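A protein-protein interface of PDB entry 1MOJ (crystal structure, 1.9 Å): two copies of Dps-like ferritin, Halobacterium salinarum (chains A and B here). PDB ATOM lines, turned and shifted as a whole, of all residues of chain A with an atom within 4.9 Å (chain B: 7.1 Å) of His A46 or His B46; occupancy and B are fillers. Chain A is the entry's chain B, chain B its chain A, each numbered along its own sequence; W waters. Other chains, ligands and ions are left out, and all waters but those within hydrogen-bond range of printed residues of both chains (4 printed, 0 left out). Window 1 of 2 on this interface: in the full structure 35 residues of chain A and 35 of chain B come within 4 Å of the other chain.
Water W3 bridges the backbone carbonyl oxygen (O) of Ala B94 (2.6 Å) and a ring nitrogen (ND1) of His A46 (2.7 Å).
Water W1 bridges the side-chain amino group (NZ) of Lys B49 (2.7 Å) and the side-chain hydroxyl (OH) of Tyr A42 (3.0 Å).
Water W2 bridges NZ of Lys A49 and OH of Tyr B42.
Water W4 lies within hydrogen-bond range of O of Ala A94 and ND1 of His B46.
Hydrophobic or aromatic side chains of chain A that line the printed part of chain B: Tyr A42, Tyr A45, His A46, Ala A94, Pro A96 and Leu A99.
Along chain A the printed residues that touch a printed residue of chain B span positions 42 to 99.
Of the 21 printed residues of chain B, 9 touch a printed residue of chain A.
Among the printed residues, no Asp or Glu carboxylate lies within 4 Å of a Lys or Arg side-chain nitrogen of the other chain.
The side-chain hydroxyl of Tyr B42 is in hydrogen-bond range of the side-chain hydroxyl of Tyr A45, 2.7 Å away.
The side-chain hydroxyl (OH) of Tyr A42 is in hydrogen-bond range of the side-chain hydroxyl (OH) of Tyr B45.
A ring nitrogen (NE2) of His B46 lies within hydrogen-bond range of a ring nitrogen (NE2) of His A46 (2.7 Å).
Among the printed residues, pairs that only touch across the chains: Tyr A42 with Lys B49 (3.1 Å), Lys A49 with Tyr B42 (3.1 Å), Pro A96 with Pro B96 (3.1 Å), His A46 with Tyr B42 (3.5 Å), Tyr A42 with His B46 (3.5 Å), His A46 with Leu B99 (3.5 Å), Leu A99 with His B46 (3.5 Å), Ala A94 with Lys B50 (3.6 Å), Lys A50 with Ala B94 (3.6 Å), Ala A94 with His B46 (3.6 Å), His A46 with Ala B94 (3.7 Å), His A46 with Pro B96 (3.7 Å), Pro A96 with His B46 (3.7 Å) and Tyr A42 with Trp B53 (3.8 Å).
His A46 touches just these residues of chain B: Tyr B42, His B46, Ala B94, Pro B96 and Leu B99.
Printed residues of chain B within 4 Å of Lys A49: Tyr B42.
Val B41 touches none of the printed residues of chain A.
Printed residues of chain A within 4 Å of Tyr B42: Tyr A45 (2.7 Å), His A46 (3.5 Å) and Lys A49 (3.1 Å).
Printed residues of chain A within 4 Å of Tyr B45: Tyr A42 (2.6 Å).
His B46 touches just these residues of chain A: Tyr A42, His A46, Ala A94, Pro A96 and Leu A99.
The nearest printed residue of chain A that does not touch His B46 is Tyr A45 (5.0 Å).
Tyr A42 touches Tyr B45, and with the chains exchanged Tyr A45 touches Tyr B42.
Tyr A42 touches His B46, and with the chains exchanged His A46 touches Tyr B42.
His A46 touches Pro B96, and with the chains exchanged Pro A96 touches His B46.
Lys A50 touches Ala B94, and with the chains exchanged Ala A94 touches Lys B50.
Of the 17 pairs that touch across the chains among the printed residues, 16 have their exchanged pair printed and touching as well.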
ATOM      1  N   TYR A  42      17.924   7.684  31.249  1.00  0.00           N
ATOM      2  CA  TYR A  42      19.126   8.133  30.571  1.00  0.00           C
ATOM      3  C   TYR A  42      19.535   9.560  30.959  1.00  0.00           C
ATOM      4  O   TYR A  42      20.721   9.890  30.937  1.00  0.00           O
ATOM      5  CB  TYR A  42      18.971   7.989  29.060  1.00  0.00           C
ATOM      6  CG  TYR A  42      19.925   6.975  28.485  1.00  0.00           C
ATOM      7  CD1 TYR A  42      19.506   6.050  27.528  1.00  0.00           C
ATOM      8  CD2 TYR A  42      21.260   6.930  28.909  1.00  0.00           C
ATOM      9  CE1 TYR A  42      20.393   5.099  27.006  1.00  0.00           C
ATOM     10  CE2 TYR A  42      22.151   5.992  28.398  1.00  0.00           C
ATOM     11  CZ  TYR A  42      21.711   5.076  27.446  1.00  0.00           C
ATOM     12  OH  TYR A  42      22.596   4.144  26.945  1.00  0.00           O
ATOM     13  N   VAL A  43      18.572  10.416  31.311  1.00  0.00           N
ATOM     14  CA  VAL A  43      18.952  11.766  31.726  1.00  0.00           C
ATOM     15  C   VAL A  43      19.579  11.591  33.103  1.00  0.00           C
ATOM     16  O   VAL A  43      20.554  12.261  33.429  1.00  0.00           O
ATOM     17  CB  VAL A  43      17.749  12.756  31.812  1.00  0.00           C
ATOM     18  CG1 VAL A  43      17.041  12.845  30.468  1.00  0.00           C
ATOM     19  CG2 VAL A  43      16.803  12.330  32.884  1.00  0.00           C
ATOM     20  N   LEU A  44      19.019  10.675  33.899  1.00  0.00           N
ATOM     21  CA  LEU A  44      19.555  10.380  35.231  1.00  0.00           C
ATOM     22  C   LEU A  44      21.000   9.913  35.073  1.00  0.00           C
ATOM     23  O   LEU A  44      21.900  10.384  35.765  1.00  0.00           O
ATOM     24  CB  LEU A  44      18.741   9.276  35.909  1.00  0.00           C
ATOM     25  CG  LEU A  44      19.345   8.677  37.190  1.00  0.00           C
ATOM     26  CD1 LEU A  44      19.444   9.748  38.271  1.00  0.00           C
ATOM     27  CD2 LEU A  44      18.497   7.515  37.670  1.00  0.00           C
ATOM     28  N   TYR A  45      21.211   8.981  34.151  1.00  0.00           N
ATOM     29  CA  TYR A  45      22.540   8.448  33.864  1.00  0.00           C
ATOM     30  C   TYR A  45      23.529   9.579  33.584  1.00  0.00           C
ATOM     31  O   TYR A  45      24.606   9.657  34.186  1.00  0.00           O
ATOM     32  CB  TYR A  45      22.470   7.525  32.647  1.00  0.00           C
ATOM     33  CG  TYR A  45      23.803   7.311  31.965  1.00  0.00           C
ATOM     34  CD1 TYR A  45      24.749   6.439  32.494  1.00  0.00           C
ATOM     35  CD2 TYR A  45      24.112   7.983  30.785  1.00  0.00           C
ATOM     36  CE1 TYR A  45      25.980   6.238  31.856  1.00  0.00           C
ATOM     37  CE2 TYR A  45      25.332   7.795  30.140  1.00  0.00           C
ATOM     38  CZ  TYR A  45      26.263   6.917  30.682  1.00  0.00           C
ATOM     39  OH  TYR A  45      27.460   6.723  30.046  1.00  0.00           O
ATOM     40  N   HIS A  46      23.160  10.460  32.662  1.00  0.00           N
ATOM     41  CA  HIS A  46      24.025  11.582  32.313  1.00  0.00           C
ATOM     42  C   HIS A  46      24.270  12.571  33.441  1.00  0.00           C
ATOM     43  O   HIS A  46      25.355  13.159  33.525  1.00  0.00           O
ATOM     44  CB  HIS A  46      23.467  12.302  31.087  1.00  0.00           C
ATOM     45  CG  HIS A  46      23.852  11.649  29.797  1.00  0.00           C
ATOM     46  ND1 HIS A  46      25.134  11.699  29.296  1.00  0.00           N
ATOM     47  CD2 HIS A  46      23.140  10.888  28.934  1.00  0.00           C
ATOM     48  CE1 HIS A  46      25.196  10.994  28.181  1.00  0.00           C
ATOM     49  NE2 HIS A  46      24.000  10.490  27.941  1.00  0.00           N
ATOM     50  N   GLN A  47      23.277  12.769  34.305  1.00  0.00           N
ATOM     51  CA  GLN A  47      23.459  13.687  35.420  1.00  0.00           C
ATOM     52  C   GLN A  47      24.314  13.016  36.499  1.00  0.00           C
ATOM     53  O   GLN A  47      25.100  13.674  37.174  1.00  0.00           O
ATOM     54  CB  GLN A  47      22.107  14.135  35.995  1.00  0.00           C
ATOM     55  CG  GLN A  47      22.256  15.274  37.012  1.00  0.00           C
ATOM     56  CD  GLN A  47      21.053  16.209  37.044  1.00  0.00           C
ATOM     57  OE1 GLN A  47      20.792  16.941  36.083  1.00  0.00           O
ATOM     58  NE2 GLN A  47      20.316  16.186  38.149  1.00  0.00           N
ATOM     59  N   LEU A  48      24.164  11.701  36.659  1.00  0.00           N
ATOM     60  CA  LEU A  48      24.966  10.977  37.634  1.00  0.00           C
ATOM     61  C   LEU A  48      26.409  11.025  37.160  1.00  0.00           C
ATOM     62  O   LEU A  48      27.339  11.144  37.964  1.00  0.00           O
ATOM     63  CB  LEU A  48      24.500   9.532  37.745  1.00  0.00           C
ATOM     64  CG  LEU A  48      23.188   9.329  38.497  1.00  0.00           C
ATOM     65  CD1 LEU A  48      22.779   7.868  38.415  1.00  0.00           C
ATOM     66  CD2 LEU A  48      23.353   9.759  39.945  1.00  0.00           C
ATOM     67  N   LYS A  49      26.602  10.923  35.847  1.00  0.00           N
ATOM     68  CA  LYS A  49      27.951  10.987  35.279  1.00  0.00           C
ATOM     69  C   LYS A  49      28.522  12.368  35.576  1.00  0.00           C
ATOM     70  O   LYS A  49      29.660  12.497  36.006  1.00  0.00           O
ATOM     71  CB  LYS A  49      27.914  10.763  33.772  1.00  0.00           C
ATOM     72  CG  LYS A  49      27.482   9.370  33.401  1.00  0.00           C
ATOM     73  CD  LYS A  49      28.586   8.579  32.735  1.00  0.00           C
ATOM     74  CE  LYS A  49      29.783   8.402  33.629  1.00  0.00           C
ATOM     75  NZ  LYS A  49      30.699   7.376  33.039  1.00  0.00           N
ATOM     76  N   LYS A  50      27.717  13.400  35.344  1.00  0.00           N
ATOM     77  CA  LYS A  50      28.135  14.774  35.602  1.00  0.00           C
ATOM     78  C   LYS A  50      28.632  14.957  37.028  1.00  0.00           C
ATOM     79  O   LYS A  50      29.703  15.505  37.253  1.00  0.00           O
ATOM     80  CB  LYS A  50      26.980  15.742  35.368  1.00  0.00           C
ATOM     81  CG  LYS A  50      27.319  17.186  35.715  1.00  0.00           C
ATOM     82  CD  LYS A  50      26.073  18.067  35.647  1.00  0.00           C
ATOM     83  CE  LYS A  50      26.392  19.556  35.833  1.00  0.00           C
ATOM     84  NZ  LYS A  50      25.147  20.383  35.752  1.00  0.00           N
ATOM     85  N   ALA A  94      16.449   7.185  21.154  1.00  0.00           N
ATOM     86  CA  ALA A  94      17.879   6.983  21.021  1.00  0.00           C
ATOM     87  C   ALA A  94      18.766   8.213  21.148  1.00  0.00           C
ATOM     88  O   ALA A  94      19.644   8.260  22.007  1.00  0.00           O
ATOM     89  CB  ALA A  94      18.160   6.280  19.702  1.00  0.00           C
ATOM     90  N   PRO A  96      20.431  11.762  22.090  1.00  0.00           N
ATOM     91  CA  PRO A  96      20.518  12.516  23.344  1.00  0.00           C
ATOM     92  C   PRO A  96      19.402  13.553  23.416  1.00  0.00           C
ATOM     93  O   PRO A  96      18.756  13.728  24.454  1.00  0.00           O
ATOM     94  CB  PRO A  96      21.896  13.168  23.251  1.00  0.00           C
ATOM     95  CG  PRO A  96      22.680  12.167  22.458  1.00  0.00           C
ATOM     96  CD  PRO A  96      21.723  11.768  21.383  1.00  0.00           C
ATOM     97  N   LEU A  99      16.067  11.806  23.963  1.00  0.00           N
ATOM     98  CA  LEU A  99      15.985  11.315  25.323  1.00  0.00           C
ATOM     99  C   LEU A  99      15.619  12.442  26.277  1.00  0.00           C
ATOM    100  O   LEU A  99      14.677  12.316  27.054  1.00  0.00           O
ATOM    101  CB  LEU A  99      17.306  10.660  25.725  1.00  0.00           C
ATOM    102  CG  LEU A  99      17.561   9.309  25.032  1.00  0.00           C
ATOM    103  CD1 LEU A  99      19.024   8.931  25.146  1.00  0.00           C
ATOM    104  CD2 LEU A  99      16.676   8.226  25.651  1.00  0.00           C
ATOM    105  N   ASN B  40      30.965  14.686  20.658  1.00  0.00           N
ATOM    106  CA  ASN B  40      30.874  13.769  19.529  1.00  0.00           C
ATOM    107  C   ASN B  40      30.913  12.323  19.968  1.00  0.00           C
ATOM    108  O   ASN B  40      30.175  11.497  19.429  1.00  0.00           O
ATOM    109  CB  ASN B  40      32.000  14.018  18.526  1.00  0.00           C
ATOM    110  CG  ASN B  40      31.814  15.311  17.759  1.00  0.00           C
ATOM    111  OD1 ASN B  40      30.684  15.702  17.452  1.00  0.00           O
ATOM    112  ND2 ASN B  40      32.915  15.972  17.434  1.00  0.00           N
ATOM    113  N   VAL B  41      31.770  12.018  20.942  1.00  0.00           N
ATOM    114  CA  VAL B  41      31.901  10.650  21.421  1.00  0.00           C
ATOM    115  C   VAL B  41      30.619  10.176  22.088  1.00  0.00           C
ATOM    116  O   VAL B  41      30.232   9.018  21.933  1.00  0.00           O
ATOM    117  CB  VAL B  41      33.089  10.499  22.399  1.00  0.00           C
ATOM    118  CG1 VAL B  41      33.098   9.103  23.007  1.00  0.00           C
ATOM    119  CG2 VAL B  41      34.397  10.715  21.651  1.00  0.00           C
ATOM    120  N   TYR B  42      29.943  11.063  22.813  1.00  0.00           N
ATOM    121  CA  TYR B  42      28.710  10.661  23.465  1.00  0.00           C
ATOM    122  C   TYR B  42      27.547  10.488  22.491  1.00  0.00           C
ATOM    123  O   TYR B  42      26.673   9.657  22.725  1.00  0.00           O
ATOM    124  CB  TYR B  42      28.346  11.630  24.589  1.00  0.00           C
ATOM    125  CG  TYR B  42      28.394  10.965  25.943  1.00  0.00           C
ATOM    126  CD1 TYR B  42      28.994  11.597  27.032  1.00  0.00           C
ATOM    127  CD2 TYR B  42      27.873   9.683  26.124  1.00  0.00           C
ATOM    128  CE1 TYR B  42      29.081  10.970  28.276  1.00  0.00           C
ATOM    129  CE2 TYR B  42      27.956   9.041  27.360  1.00  0.00           C
ATOM    130  CZ  TYR B  42      28.562   9.692  28.432  1.00  0.00           C
ATOM    131  OH  TYR B  42      28.643   9.069  29.651  1.00  0.00           O
ATOM    132  N   VAL B  43      27.520  11.258  21.403  1.00  0.00           N
ATOM    133  CA  VAL B  43      26.446  11.069  20.429  1.00  0.00           C
ATOM    134  C   VAL B  43      26.740   9.737  19.742  1.00  0.00           C
ATOM    135  O   VAL B  43      25.825   8.981  19.429  1.00  0.00           O
ATOM    136  CB  VAL B  43      26.377  12.197  19.354  1.00  0.00           C
ATOM    137  CG1 VAL B  43      26.215  13.560  20.017  1.00  0.00           C
ATOM    138  CG2 VAL B  43      27.592  12.165  18.494  1.00  0.00           C
ATOM    139  N   LEU B  44      28.023   9.452  19.512  1.00  0.00           N
ATOM    140  CA  LEU B  44      28.426   8.189  18.902  1.00  0.00           C
ATOM    141  C   LEU B  44      27.936   7.056  19.795  1.00  0.00           C
ATOM    142  O   LEU B  44      27.309   6.092  19.324  1.00  0.00           O
ATOM    143  CB  LEU B  44      29.948   8.108  18.773  1.00  0.00           C
ATOM    144  CG  LEU B  44      30.527   6.727  18.400  1.00  0.00           C
ATOM    145  CD1 LEU B  44      30.071   6.329  17.017  1.00  0.00           C
ATOM    146  CD2 LEU B  44      32.038   6.757  18.460  1.00  0.00           C
ATOM    147  N   TYR B  45      28.233   7.181  21.086  1.00  0.00           N
ATOM    148  CA  TYR B  45      27.828   6.188  22.081  1.00  0.00           C
ATOM    149  C   TYR B  45      26.332   5.898  21.976  1.00  0.00           C
ATOM    150  O   TYR B  45      25.909   4.738  21.914  1.00  0.00           O
ATOM    151  CB  TYR B  45      28.131   6.705  23.488  1.00  0.00           C
ATOM    152  CG  TYR B  45      27.327   6.025  24.583  1.00  0.00           C
ATOM    153  CD1 TYR B  45      27.668   4.759  25.046  1.00  0.00           C
ATOM    154  CD2 TYR B  45      26.229   6.663  25.159  1.00  0.00           C
ATOM    155  CE1 TYR B  45      26.937   4.145  26.061  1.00  0.00           C
ATOM    156  CE2 TYR B  45      25.494   6.061  26.169  1.00  0.00           C
ATOM    157  CZ  TYR B  45      25.853   4.804  26.617  1.00  0.00           C
ATOM    158  OH  TYR B  45      25.126   4.212  27.628  1.00  0.00           O
ATOM    159  N   HIS B  46      25.531   6.961  21.967  1.00  0.00           N
ATOM    160  CA  HIS B  46      24.086   6.803  21.895  1.00  0.00           C
ATOM    161  C   HIS B  46      23.593   6.207  20.585  1.00  0.00           C
ATOM    162  O   HIS B  46      22.601   5.464  20.574  1.00  0.00           O
ATOM    163  CB  HIS B  46      23.404   8.139  22.173  1.00  0.00           C
ATOM    164  CG  HIS B  46      23.241   8.424  23.631  1.00  0.00           C
ATOM    165  ND1 HIS B  46      22.322   7.758  24.414  1.00  0.00           N
ATOM    166  CD2 HIS B  46      23.912   9.258  24.460  1.00  0.00           C
ATOM    167  CE1 HIS B  46      22.439   8.167  25.666  1.00  0.00           C
ATOM    168  NE2 HIS B  46      23.397   9.075  25.721  1.00  0.00           N
ATOM    169  N   GLN B  47      24.278   6.507  19.486  1.00  0.00           N
ATOM    170  CA  GLN B  47      23.862   5.949  18.206  1.00  0.00           C
ATOM    171  C   GLN B  47      24.297   4.484  18.125  1.00  0.00           C
ATOM    172  O   GLN B  47      23.602   3.648  17.548  1.00  0.00           O
ATOM    173  CB  GLN B  47      24.445   6.750  17.043  1.00  0.00           C
ATOM    174  CG  GLN B  47      23.839   6.351  15.702  1.00  0.00           C
ATOM    175  CD  GLN B  47      23.789   7.495  14.704  1.00  0.00           C
ATOM    176  OE1 GLN B  47      23.018   8.447  14.864  1.00  0.00           O
ATOM    177  NE2 GLN B  47      24.614   7.407  13.667  1.00  0.00           N
ATOM    178  N   LEU B  48      25.446   4.173  18.713  1.00  0.00           N
ATOM    179  CA  LEU B  48      25.915   2.796  18.727  1.00  0.00           C
ATOM    180  C   LEU B  48      24.933   1.989  19.561  1.00  0.00           C
ATOM    181  O   LEU B  48      24.636   0.849  19.237  1.00  0.00           O
ATOM    182  CB  LEU B  48      27.316   2.701  19.331  1.00  0.00           C
ATOM    183  CG  LEU B  48      28.454   3.188  18.435  1.00  0.00           C
ATOM    184  CD1 LEU B  48      29.747   3.185  19.200  1.00  0.00           C
ATOM    185  CD2 LEU B  48      28.553   2.301  17.221  1.00  0.00           C
ATOM    186  N   LYS B  49      24.436   2.578  20.646  1.00  0.00           N
ATOM    187  CA  LYS B  49      23.470   1.898  21.498  1.00  0.00           C
ATOM    188  C   LYS B  49      22.216   1.648  20.682  1.00  0.00           C
ATOM    189  O   LYS B  49      21.653   0.554  20.709  1.00  0.00           O
ATOM    190  CB  LYS B  49      23.119   2.758  22.707  1.00  0.00           C
ATOM    191  CG  LYS B  49      24.266   2.958  23.659  1.00  0.00           C
ATOM    192  CD  LYS B  49      24.037   2.276  24.997  1.00  0.00           C
ATOM    193  CE  LYS B  49      23.852   0.788  24.871  1.00  0.00           C
ATOM    194  NZ  LYS B  49      23.939   0.143  26.222  1.00  0.00           N
ATOM    195  N   LYS B  50      21.783   2.675  19.954  1.00  0.00           N
ATOM    196  CA  LYS B  50      20.593   2.568  19.118  1.00  0.00           C
ATOM    197  C   LYS B  50      20.692   1.392  18.152  1.00  0.00           C
ATOM    198  O   LYS B  50      19.772   0.581  18.047  1.00  0.00           O
ATOM    199  CB  LYS B  50      20.386   3.854  18.309  1.00  0.00           C
ATOM    200  CG  LYS B  50      19.228   3.775  17.310  1.00  0.00           C
ATOM    201  CD  LYS B  50      19.180   5.007  16.426  1.00  0.00           C
ATOM    202  CE  LYS B  50      17.942   5.012  15.515  1.00  0.00           C
ATOM    203  NZ  LYS B  50      17.933   6.228  14.652  1.00  0.00           N
ATOM    204  N   HIS B  51      21.804   1.307  17.441  1.00  0.00           N
ATOM    205  CA  HIS B  51      22.002   0.242  16.468  1.00  0.00           C
ATOM    206  C   HIS B  51      22.147  -1.111  17.128  1.00  0.00           C
ATOM    207  O   HIS B  51      21.717  -2.124  16.586  1.00  0.00           O
ATOM    208  CB  HIS B  51      23.200   0.590  15.599  1.00  0.00           C
ATOM    209  CG  HIS B  51      22.996   1.845  14.811  1.00  0.00           C
ATOM    210  ND1 HIS B  51      24.032   2.551  14.245  1.00  0.00           N
ATOM    211  CD2 HIS B  51      21.867   2.529  14.514  1.00  0.00           C
ATOM    212  CE1 HIS B  51      23.552   3.620  13.633  1.00  0.00           C
ATOM    213  NE2 HIS B  51      22.240   3.629  13.782  1.00  0.00           N
ATOM    214  N   HIS B  52      22.747  -1.106  18.310  1.00  0.00           N
ATOM    215  CA  HIS B  52      22.924  -2.301  19.130  1.00  0.00           C
ATOM    216  C   HIS B  52      21.518  -2.848  19.457  1.00  0.00           C
ATOM    217  O   HIS B  52      21.232  -4.035  19.259  1.00  0.00           O
ATOM    218  CB  HIS B  52      23.665  -1.876  20.405  1.00  0.00           C
ATOM    219  CG  HIS B  52      23.582  -2.854  21.535  1.00  0.00           C
ATOM    220  ND1 HIS B  52      24.272  -4.047  21.549  1.00  0.00           N
ATOM    221  CD2 HIS B  52      22.958  -2.769  22.734  1.00  0.00           C
ATOM    222  CE1 HIS B  52      24.083  -4.652  22.709  1.00  0.00           C
ATOM    223  NE2 HIS B  52      23.288  -3.896  23.445  1.00  0.00           N
ATOM    224  N   TRP B  53      20.639  -1.970  19.939  1.00  0.00           N
ATOM    225  CA  TRP B  53      19.277  -2.364  20.295  1.00  0.00           C
ATOM    226  C   TRP B  53      18.458  -2.842  19.106  1.00  0.00           C
ATOM    227  O   TRP B  53      17.801  -3.864  19.179  1.00  0.00           O
ATOM    228  CB  TRP B  53      18.495  -1.201  20.932  1.00  0.00           C
ATOM    229  CG  TRP B  53      19.083  -0.602  22.185  1.00  0.00           C
ATOM    230  CD1 TRP B  53      19.739  -1.265  23.195  1.00  0.00           C
ATOM    231  CD2 TRP B  53      19.021   0.778  22.586  1.00  0.00           C
ATOM    232  NE1 TRP B  53      20.086  -0.378  24.198  1.00  0.00           N
ATOM    233  CE2 TRP B  53      19.664   0.879  23.848  1.00  0.00           C
ATOM    234  CE3 TRP B  53      18.493   1.937  22.000  1.00  0.00           C
ATOM    235  CZ2 TRP B  53      19.784   2.093  24.530  1.00  0.00           C
ATOM    236  CZ3 TRP B  53      18.614   3.142  22.679  1.00  0.00           C
ATOM    237  CH2 TRP B  53      19.259   3.212  23.930  1.00  0.00           C
ATOM    238  N   ALA B  71      29.864   0.551  21.881  1.00  0.00           N
ATOM    239  CA  ALA B  71      29.238   1.566  22.721  1.00  0.00           C
ATOM    240  C   ALA B  71      29.982   1.662  24.046  1.00  0.00           C
ATOM    241  O   ALA B  71      30.287   2.754  24.533  1.00  0.00           O
ATOM    242  CB  ALA B  71      27.767   1.225  22.956  1.00  0.00           C
ATOM    243  N   ALA B  74      33.091   3.586  23.528  1.00  0.00           N
ATOM    244  CA  ALA B  74      32.806   5.002  23.324  1.00  0.00           C
ATOM    245  C   ALA B  74      32.473   5.661  24.652  1.00  0.00           C
ATOM    246  O   ALA B  74      32.864   6.805  24.914  1.00  0.00           O
ATOM    247  CB  ALA B  74      31.646   5.177  22.341  1.00  0.00           C
ATOM    248  N   HIS B  93      30.761  18.888  29.115  1.00  0.00           N
ATOM    249  CA  HIS B  93      29.371  18.940  28.657  1.00  0.00           C
ATOM    250  C   HIS B  93      28.703  17.761  29.327  1.00  0.00           C
ATOM    251  O   HIS B  93      29.236  16.646  29.308  1.00  0.00           O
ATOM    252  CB  HIS B  93      29.294  18.802  27.134  1.00  0.00           C
ATOM    253  CG  HIS B  93      29.983  19.906  26.400  1.00  0.00           C
ATOM    254  ND1 HIS B  93      29.785  21.237  26.703  1.00  0.00           N
ATOM    255  CD2 HIS B  93      30.873  19.882  25.381  1.00  0.00           C
ATOM    256  CE1 HIS B  93      30.526  21.985  25.905  1.00  0.00           C
ATOM    257  NE2 HIS B  93      31.198  21.188  25.093  1.00  0.00           N
ATOM    258  N   ALA B  94      27.546  17.992  29.921  1.00  0.00           N
ATOM    259  CA  ALA B  94      26.886  16.919  30.636  1.00  0.00           C
ATOM    260  C   ALA B  94      25.513  16.486  30.142  1.00  0.00           C
ATOM    261  O   ALA B  94      25.321  15.322  29.819  1.00  0.00           O
ATOM    262  CB  ALA B  94      26.815  17.287  32.118  1.00  0.00           C
ATOM    263  N   SER B  95      24.552  17.405  30.095  1.00  0.00           N
ATOM    264  CA  SER B  95      23.208  17.029  29.679  1.00  0.00           C
ATOM    265  C   SER B  95      23.182  16.505  28.253  1.00  0.00           C
ATOM    266  O   SER B  95      24.012  16.881  27.423  1.00  0.00           O
ATOM    267  CB  SER B  95      22.220  18.204  29.821  1.00  0.00           C
ATOM    268  OG  SER B  95      22.395  19.179  28.809  1.00  0.00           O
ATOM    269  N   PRO B  96      22.231  15.604  27.965  1.00  0.00           N
ATOM    270  CA  PRO B  96      22.050  14.994  26.643  1.00  0.00           C
ATOM    271  C   PRO B  96      21.885  16.083  25.587  1.00  0.00           C
ATOM    272  O   PRO B  96      22.469  16.025  24.498  1.00  0.00           O
ATOM    273  CB  PRO B  96      20.776  14.177  26.818  1.00  0.00           C
ATOM    274  CG  PRO B  96      20.855  13.761  28.252  1.00  0.00           C
ATOM    275  CD  PRO B  96      21.289  15.027  28.941  1.00  0.00           C
ATOM    276  N   LEU B  99      25.233  17.853  25.038  1.00  0.00           N
ATOM    277  CA  LEU B  99      26.136  16.983  24.308  1.00  0.00           C
ATOM    278  C   LEU B  99      25.815  17.001  22.819  1.00  0.00           C
ATOM    279  O   LEU B  99      26.707  17.223  22.001  1.00  0.00           O
ATOM    280  CB  LEU B  99      26.050  15.563  24.859  1.00  0.00           C
ATOM    281  CG  LEU B  99      26.673  15.418  26.257  1.00  0.00           C
ATOM    282  CD1 LEU B  99      26.228  14.113  26.890  1.00  0.00           C
ATOM    283  CD2 LEU B  99      28.204  15.488  26.157  1.00  0.00           C
HETATM  284  O   HOH W   1      22.078   1.329  27.787  1.00  0.00           O
HETATM  285  O   HOH W   2      31.399   8.115  30.505  1.00  0.00           O
HETATM  286  O   HOH W   3      26.579  13.314  30.895  1.00  0.00           O
HETATM  287  O   HOH W   4      20.712   5.927  23.015  1.00  0.00           O
